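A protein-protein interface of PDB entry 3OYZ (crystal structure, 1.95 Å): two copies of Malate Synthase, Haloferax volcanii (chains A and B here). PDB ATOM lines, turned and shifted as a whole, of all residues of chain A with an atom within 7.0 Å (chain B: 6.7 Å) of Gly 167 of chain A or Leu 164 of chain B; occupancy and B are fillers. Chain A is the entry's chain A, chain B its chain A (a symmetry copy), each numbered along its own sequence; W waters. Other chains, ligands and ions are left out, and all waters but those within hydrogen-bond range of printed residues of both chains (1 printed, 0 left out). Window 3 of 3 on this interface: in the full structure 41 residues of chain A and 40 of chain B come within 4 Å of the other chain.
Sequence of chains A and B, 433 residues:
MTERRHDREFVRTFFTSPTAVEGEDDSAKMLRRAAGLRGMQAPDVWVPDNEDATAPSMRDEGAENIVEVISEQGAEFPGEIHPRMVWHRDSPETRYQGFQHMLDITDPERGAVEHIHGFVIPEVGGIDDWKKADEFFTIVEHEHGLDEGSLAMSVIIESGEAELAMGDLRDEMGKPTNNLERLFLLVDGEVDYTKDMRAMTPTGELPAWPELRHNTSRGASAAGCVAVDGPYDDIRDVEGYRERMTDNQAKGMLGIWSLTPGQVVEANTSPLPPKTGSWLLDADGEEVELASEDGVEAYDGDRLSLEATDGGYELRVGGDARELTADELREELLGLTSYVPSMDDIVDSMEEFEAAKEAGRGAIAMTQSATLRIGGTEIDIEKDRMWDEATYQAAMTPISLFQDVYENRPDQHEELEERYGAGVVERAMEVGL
The side-chain carboxylate of Glu 161 of chain B is in salt-bridge range of the guanidinium group of Arg 170 of chain A, 2.9 Å away.
NH1 of Arg 218 of chain A lies within salt-bridge range of OE2 of Glu 163 of chain B (3.3 Å).
The guanidinium group (NE) of Arg 170 of chain A lies within salt-bridge range of the side-chain carboxylate (OD1) of Asp 171 of chain A (3.1 Å).
OD1 of Asn 215 of chain A sits close to NH2 of Arg 218 of chain A (3.4 Å).
Leu 164 of chain B touches Gly 167 of chain A (CD1 to O, 3.8 Å).
Gly 126 of chain B touches Arg 170 of chain A.
NE of Arg 218 of chain A touches CD2 of Leu 164 of chain B, 3.5 Å away.
CG of Glu 161 of chain B touches O of Ala 222 of chain A, at 3.9 Å.
Leu 164 of chain B touches Ala 222 of chain A.
Gly 167 of chain A touches just one residue of chain B: Leu 164 (3.8 Å).
Of the printed residues of chain A, Leu 164 of chain B touches Gly 167, Arg 218 and Ala 222.
Printed residues of chain A within 4 Å of Gly 126 of chain B: Arg 170.
Of the printed residues of chain B, Arg 218 of chain A touches Glu 163 (3.2 Å) and Leu 164 (3.5 Å).
Of the printed residues of chain B, Ala 222 of chain A touches Glu 161 (3.9 Å) and Leu 164 (3.8 Å).
The nearest printed residue of chain A that does not touch Glu 163 of chain B is Asn 215 of chain A (5.3 Å).
Hydrophobic or aromatic side chains of chain B within 4 Å of the printed part of chain A: Leu 164.
Along chain B the printed residues that touch a printed residue of chain A span positions 126 to 164.
Of the 15 printed residues of chain A, 4 touch a printed residue of chain B.
Among the printed residues, 7 pairs touch across the chains.
Among the printed residues, Asp or Glu carboxylates within 4 Å of a Lys or Arg side-chain nitrogen of the other chain: Arg 170 of chain A with Glu 161 of chain B (2.9 Å) and Arg 218 of chain A with Glu 163 of chain B (3.3 Å).
Gly 167 of chain A touches Leu 164 of chain B, but with the chains exchanged Leu 164 of chain A does not touch Gly 167 of chain B (10.3 Å).
Positions printed for both chains: 162, 163, 164, 165, 166, 167 and 168.
Of the 7 pairs that touch across the chains among the printed residues, none has its exchanged pair printed and touching as well.
Water W1 bridges O of Glu 161 of chain B (2.7 Å) and NH1 of Arg 170 of chain A (2.9 Å).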
ATOM      1  N   ALA A 162      21.986  19.152  10.202  1.00  0.00           N
ATOM      2  CA  ALA A 162      21.859  20.501  10.696  1.00  0.00           C
ATOM      3  C   ALA A 162      20.979  20.396  11.933  1.00  0.00           C
ATOM      4  O   ALA A 162      21.064  21.280  12.781  1.00  0.00           O
ATOM      5  CB  ALA A 162      21.075  21.352   9.652  1.00  0.00           C
ATOM      6  N   GLU A 163      20.010  19.492  11.927  1.00  0.00           N
ATOM      7  CA  GLU A 163      19.148  19.324  13.113  1.00  0.00           C
ATOM      8  C   GLU A 163      19.982  18.996  14.338  1.00  0.00           C
ATOM      9  O   GLU A 163      19.802  19.591  15.417  1.00  0.00           O
ATOM     10  CB  GLU A 163      18.110  18.199  12.923  1.00  0.00           C
ATOM     11  CG  GLU A 163      17.203  17.939  14.143  1.00  0.00           C
ATOM     12  CD  GLU A 163      16.261  16.774  13.842  1.00  0.00           C
ATOM     13  OE1 GLU A 163      16.361  16.271  12.709  1.00  0.00           O
ATOM     14  OE2 GLU A 163      15.441  16.295  14.661  1.00  0.00           O
ATOM     15  N   LEU A 164      20.902  18.046  14.185  1.00  0.00           N
ATOM     16  CA  LEU A 164      21.854  17.748  15.303  1.00  0.00           C
ATOM     17  C   LEU A 164      22.779  18.926  15.646  1.00  0.00           C
ATOM     18  O   LEU A 164      23.085  19.150  16.842  1.00  0.00           O
ATOM     19  CB  LEU A 164      22.730  16.535  14.925  1.00  0.00           C
ATOM     20  CG  LEU A 164      21.938  15.213  14.876  1.00  0.00           C
ATOM     21  CD1 LEU A 164      22.718  14.059  14.245  1.00  0.00           C
ATOM     22  CD2 LEU A 164      21.413  14.826  16.259  1.00  0.00           C
ATOM     23  N   ALA A 165      23.159  19.713  14.620  1.00  0.00           N
ATOM     24  CA  ALA A 165      24.089  20.827  14.891  1.00  0.00           C
ATOM     25  C   ALA A 165      23.442  21.867  15.809  1.00  0.00           C
ATOM     26  O   ALA A 165      24.136  22.641  16.485  1.00  0.00           O
ATOM     27  CB  ALA A 165      24.576  21.564  13.604  1.00  0.00           C
ATOM     28  N   MET A 166      22.129  21.861  15.978  1.00  0.00           N
ATOM     29  CA  MET A 166      21.523  22.919  16.841  1.00  0.00           C
ATOM     30  C   MET A 166      21.803  22.592  18.317  1.00  0.00           C
ATOM     31  O   MET A 166      21.758  23.510  19.153  1.00  0.00           O
ATOM     32  CB  MET A 166      20.005  23.066  16.629  1.00  0.00           C
ATOM     33  CG  MET A 166      19.610  23.615  15.294  1.00  0.00           C
ATOM     34  SD  MET A 166      17.809  23.780  15.178  1.00  0.00           S
ATOM     35  CE  MET A 166      17.255  22.120  14.834  1.00  0.00           C
ATOM     36  N   GLY A 167      22.198  21.349  18.626  1.00  0.00           N
ATOM     37  CA  GLY A 167      22.428  20.896  20.023  1.00  0.00           C
ATOM     38  C   GLY A 167      23.536  21.652  20.767  1.00  0.00           C
ATOM     39  O   GLY A 167      23.478  21.803  22.001  1.00  0.00           O
ATOM     40  N   ASP A 168      24.582  22.133  20.086  1.00  0.00           N
ATOM     41  CA  ASP A 168      25.682  22.725  20.825  1.00  0.00           C
ATOM     42  C   ASP A 168      25.955  24.199  20.391  1.00  0.00           C
ATOM     43  O   ASP A 168      27.081  24.710  20.508  1.00  0.00           O
ATOM     44  CB  ASP A 168      26.928  21.835  20.709  1.00  0.00           C
ATOM     45  CG  ASP A 168      27.992  22.147  21.763  1.00  0.00           C
ATOM     46  OD1 ASP A 168      27.622  22.562  22.894  1.00  0.00           O
ATOM     47  OD2 ASP A 168      29.196  22.055  21.427  1.00  0.00           O
ATOM     48  N   LEU A 169      24.922  24.876  19.894  1.00  0.00           N
ATOM     49  CA  LEU A 169      25.100  26.125  19.213  1.00  0.00           C
ATOM     50  C   LEU A 169      25.548  27.154  20.200  1.00  0.00           C
ATOM     51  O   LEU A 169      26.412  27.972  19.880  1.00  0.00           O
ATOM     52  CB  LEU A 169      23.739  26.538  18.627  1.00  0.00           C
ATOM     53  CG  LEU A 169      23.461  27.492  17.496  1.00  0.00           C
ATOM     54  CD1 LEU A 169      24.541  27.271  16.468  1.00  0.00           C
ATOM     55  CD2 LEU A 169      22.061  27.187  16.955  1.00  0.00           C
ATOM     56  N   ARG A 170      24.965  27.154  21.404  1.00  0.00           N
ATOM     57  CA  ARG A 170      25.372  28.170  22.383  1.00  0.00           C
ATOM     58  C   ARG A 170      26.879  28.251  22.613  1.00  0.00           C
ATOM     59  O   ARG A 170      27.476  29.332  22.618  1.00  0.00           O
ATOM     60  CB  ARG A 170      24.615  27.960  23.733  1.00  0.00           C
ATOM     61  CG  ARG A 170      24.982  28.940  24.846  1.00  0.00           C
ATOM     62  CD  ARG A 170      24.551  28.348  26.255  1.00  0.00           C
ATOM     63  NE  ARG A 170      25.450  27.200  26.547  1.00  0.00           N
ATOM     64  CZ  ARG A 170      25.036  25.999  26.972  1.00  0.00           C
ATOM     65  NH1 ARG A 170      23.755  25.834  27.243  1.00  0.00           N
ATOM     66  NH2 ARG A 170      25.854  24.947  27.040  1.00  0.00           N
ATOM     67  N   ASP A 171      27.549  27.155  22.928  1.00  0.00           N
ATOM     68  CA  ASP A 171      28.967  27.272  23.100  1.00  0.00           C
ATOM     69  C   ASP A 171      29.788  27.428  21.782  1.00  0.00           C
ATOM     70  O   ASP A 171      30.851  27.985  21.827  1.00  0.00           O
ATOM     71  CB  ASP A 171      29.391  25.980  23.774  1.00  0.00           C
ATOM     72  CG  ASP A 171      28.906  25.934  25.283  1.00  0.00           C
ATOM     73  OD1 ASP A 171      28.469  26.947  25.873  1.00  0.00           O
ATOM     74  OD2 ASP A 171      28.963  24.837  25.859  1.00  0.00           O
ATOM     75  N   ASN A 215      12.597  20.261  18.113  1.00  0.00           N
ATOM     76  CA  ASN A 215      14.054  20.526  18.187  1.00  0.00           C
ATOM     77  C   ASN A 215      14.529  21.876  17.665  1.00  0.00           C
ATOM     78  O   ASN A 215      15.470  22.426  18.240  1.00  0.00           O
ATOM     79  CB  ASN A 215      14.796  19.393  17.476  1.00  0.00           C
ATOM     80  CG  ASN A 215      14.526  18.031  18.151  1.00  0.00           C
ATOM     81  OD1 ASN A 215      13.982  17.943  19.275  1.00  0.00           O
ATOM     82  ND2 ASN A 215      14.684  16.985  17.368  1.00  0.00           N
ATOM     83  N   ARG A 218      13.394  24.341  20.452  1.00  0.00           N
ATOM     84  CA  ARG A 218      14.367  24.184  21.521  1.00  0.00           C
ATOM     85  C   ARG A 218      15.693  24.801  21.188  1.00  0.00           C
ATOM     86  O   ARG A 218      16.265  25.562  21.988  1.00  0.00           O
ATOM     87  CB  ARG A 218      14.534  22.651  21.797  1.00  0.00           C
ATOM     88  CG  ARG A 218      15.674  22.344  22.749  1.00  0.00           C
ATOM     89  CD  ARG A 218      15.631  20.825  22.829  1.00  0.00           C
ATOM     90  NE  ARG A 218      16.288  20.262  21.650  1.00  0.00           N
ATOM     91  CZ  ARG A 218      16.415  18.966  21.387  1.00  0.00           C
ATOM     92  NH1 ARG A 218      15.943  18.060  22.231  1.00  0.00           N
ATOM     93  NH2 ARG A 218      17.175  18.610  20.360  1.00  0.00           N
ATOM     94  N   GLY A 219      16.150  24.559  19.967  1.00  0.00           N
ATOM     95  CA  GLY A 219      17.468  25.058  19.605  1.00  0.00           C
ATOM     96  C   GLY A 219      17.458  26.600  19.640  1.00  0.00           C
ATOM     97  O   GLY A 219      18.440  27.229  20.069  1.00  0.00           O
ATOM     98  N   ALA A 222      17.397  27.831  23.252  1.00  0.00           N
ATOM     99  CA  ALA A 222      18.691  27.686  23.960  1.00  0.00           C
ATOM    100  C   ALA A 222      19.770  28.658  23.468  1.00  0.00           C
ATOM    101  O   ALA A 222      20.704  29.032  24.202  1.00  0.00           O
ATOM    102  CB  ALA A 222      19.173  26.243  23.728  1.00  0.00           C
ATOM    103  N   ALA A 223      19.723  29.016  22.182  1.00  0.00           N
ATOM    104  CA  ALA A 223      20.822  29.802  21.602  1.00  0.00           C
ATOM    105  C   ALA A 223      20.484  31.305  21.414  1.00  0.00           C
ATOM    106  O   ALA A 223      21.286  32.044  20.808  1.00  0.00           O
ATOM    107  CB  ALA A 223      21.206  29.212  20.240  1.00  0.00           C
ATOM    108  N   GLY B 126      22.644  25.156  31.097  1.00  0.00           N
ATOM    109  CA  GLY B 126      23.567  24.121  30.565  1.00  0.00           C
ATOM    110  C   GLY B 126      24.356  23.444  31.659  1.00  0.00           C
ATOM    111  O   GLY B 126      24.280  23.844  32.852  1.00  0.00           O
ATOM    112  N   ILE B 157      13.940  20.532  34.958  1.00  0.00           N
ATOM    113  CA  ILE B 157      14.287  20.754  33.523  1.00  0.00           C
ATOM    114  C   ILE B 157      13.195  21.666  33.045  1.00  0.00           C
ATOM    115  O   ILE B 157      12.054  21.222  32.824  1.00  0.00           O
ATOM    116  CB  ILE B 157      14.217  19.408  32.691  1.00  0.00           C
ATOM    117  CG1 ILE B 157      15.144  18.329  33.360  1.00  0.00           C
ATOM    118  CG2 ILE B 157      14.665  19.713  31.219  1.00  0.00           C
ATOM    119  CD1 ILE B 157      16.640  18.760  33.598  1.00  0.00           C
ATOM    120  N   SER B 159      14.025  24.591  30.926  1.00  0.00           N
ATOM    121  CA  SER B 159      14.503  25.422  29.833  1.00  0.00           C
ATOM    122  C   SER B 159      15.034  24.517  28.698  1.00  0.00           C
ATOM    123  O   SER B 159      15.454  23.372  28.953  1.00  0.00           O
ATOM    124  CB  SER B 159      15.661  26.276  30.324  1.00  0.00           C
ATOM    125  OG  SER B 159      16.895  25.649  30.665  1.00  0.00           O
ATOM    126  N   GLY B 160      15.055  25.088  27.503  1.00  0.00           N
ATOM    127  CA  GLY B 160      15.700  24.490  26.351  1.00  0.00           C
ATOM    128  C   GLY B 160      17.146  24.111  26.657  1.00  0.00           C
ATOM    129  O   GLY B 160      17.576  23.006  26.305  1.00  0.00           O
ATOM    130  N   GLU B 161      17.905  24.949  27.360  1.00  0.00           N
ATOM    131  CA  GLU B 161      19.327  24.686  27.609  1.00  0.00           C
ATOM    132  C   GLU B 161      19.417  23.459  28.528  1.00  0.00           C
ATOM    133  O   GLU B 161      20.372  22.696  28.396  1.00  0.00           O
ATOM    134  CB  GLU B 161      20.070  25.853  28.337  1.00  0.00           C
ATOM    135  CG  GLU B 161      20.305  27.133  27.620  1.00  0.00           C
ATOM    136  CD  GLU B 161      21.133  28.142  28.483  1.00  0.00           C
ATOM    137  OE1 GLU B 161      20.448  28.993  29.099  1.00  0.00           O
ATOM    138  OE2 GLU B 161      22.397  28.060  28.598  1.00  0.00           O
ATOM    139  N   ALA B 162      18.525  23.298  29.533  1.00  0.00           N
ATOM    140  CA  ALA B 162      18.746  22.233  30.481  1.00  0.00           C
ATOM    141  C   ALA B 162      18.346  20.957  29.753  1.00  0.00           C
ATOM    142  O   ALA B 162      18.829  19.896  30.137  1.00  0.00           O
ATOM    143  CB  ALA B 162      17.759  22.403  31.675  1.00  0.00           C
ATOM    144  N   GLU B 163      17.332  21.023  28.902  1.00  0.00           N
ATOM    145  CA  GLU B 163      16.922  19.825  28.145  1.00  0.00           C
ATOM    146  C   GLU B 163      18.083  19.287  27.329  1.00  0.00           C
ATOM    147  O   GLU B 163      18.364  18.073  27.333  1.00  0.00           O
ATOM    148  CB  GLU B 163      15.752  20.116  27.183  1.00  0.00           C
ATOM    149  CG  GLU B 163      15.301  18.916  26.326  1.00  0.00           C
ATOM    150  CD  GLU B 163      14.177  19.350  25.387  1.00  0.00           C
ATOM    151  OE1 GLU B 163      13.814  20.536  25.483  1.00  0.00           O
ATOM    152  OE2 GLU B 163      13.641  18.607  24.530  1.00  0.00           O
ATOM    153  N   LEU B 164      18.766  20.181  26.619  1.00  0.00           N
ATOM    154  CA  LEU B 164      20.003  19.758  25.888  1.00  0.00           C
ATOM    155  C   LEU B 164      21.128  19.277  26.817  1.00  0.00           C
ATOM    156  O   LEU B 164      21.857  18.316  26.468  1.00  0.00           O
ATOM    157  CB  LEU B 164      20.537  20.940  25.048  1.00  0.00           C
ATOM    158  CG  LEU B 164      19.619  21.296  23.861  1.00  0.00           C
ATOM    159  CD1 LEU B 164      19.983  22.621  23.190  1.00  0.00           C
ATOM    160  CD2 LEU B 164      19.565  20.161  22.839  1.00  0.00           C
ATOM    161  N   ALA B 165      21.222  19.886  28.016  1.00  0.00           N
ATOM    162  CA  ALA B 165      22.318  19.494  28.923  1.00  0.00           C
ATOM    163  C   ALA B 165      22.165  18.038  29.368  1.00  0.00           C
ATOM    164  O   ALA B 165      23.141  17.389  29.772  1.00  0.00           O
ATOM    165  CB  ALA B 165      22.414  20.378  30.207  1.00  0.00           C
ATOM    166  N   MET B 166      21.003  17.425  29.205  1.00  0.00           N
ATOM    167  CA  MET B 166      20.871  16.021  29.694  1.00  0.00           C
ATOM    168  C   MET B 166      21.604  15.076  28.727  1.00  0.00           C
ATOM    169  O   MET B 166      21.966  13.962  29.139  1.00  0.00           O
ATOM    170  CB  MET B 166      19.404  15.572  29.833  1.00  0.00           C
ATOM    171  CG  MET B 166      18.640  16.259  30.922  1.00  0.00           C
ATOM    172  SD  MET B 166      16.947  15.621  31.015  1.00  0.00           S
ATOM    173  CE  MET B 166      16.107  16.458  29.683  1.00  0.00           C
ATOM    174  N   GLY B 167      21.924  15.539  27.511  1.00  0.00           N
ATOM    175  CA  GLY B 167      22.569  14.698  26.468  1.00  0.00           C
ATOM    176  C   GLY B 167      23.951  14.152  26.849  1.00  0.00           C
ATOM    177  O   GLY B 167      24.345  13.062  26.398  1.00  0.00           O
ATOM    178  N   ASP B 168      24.745  14.864  27.655  1.00  0.00           N
ATOM    179  CA  ASP B 168      26.097  14.396  27.893  1.00  0.00           C
ATOM    180  C   ASP B 168      26.383  14.171  29.411  1.00  0.00           C
ATOM    181  O   ASP B 168      27.533  14.253  29.872  1.00  0.00           O
ATOM    182  CB  ASP B 168      27.105  15.352  27.238  1.00  0.00           C
ATOM    183  CG  ASP B 168      28.499  14.742  27.079  1.00  0.00           C
ATOM    184  OD1 ASP B 168      28.600  13.500  26.890  1.00  0.00           O
ATOM    185  OD2 ASP B 168      29.490  15.495  27.227  1.00  0.00           O
HETATM  186  O   HOH W   1      22.685  23.110  27.052  1.00  0.00           O
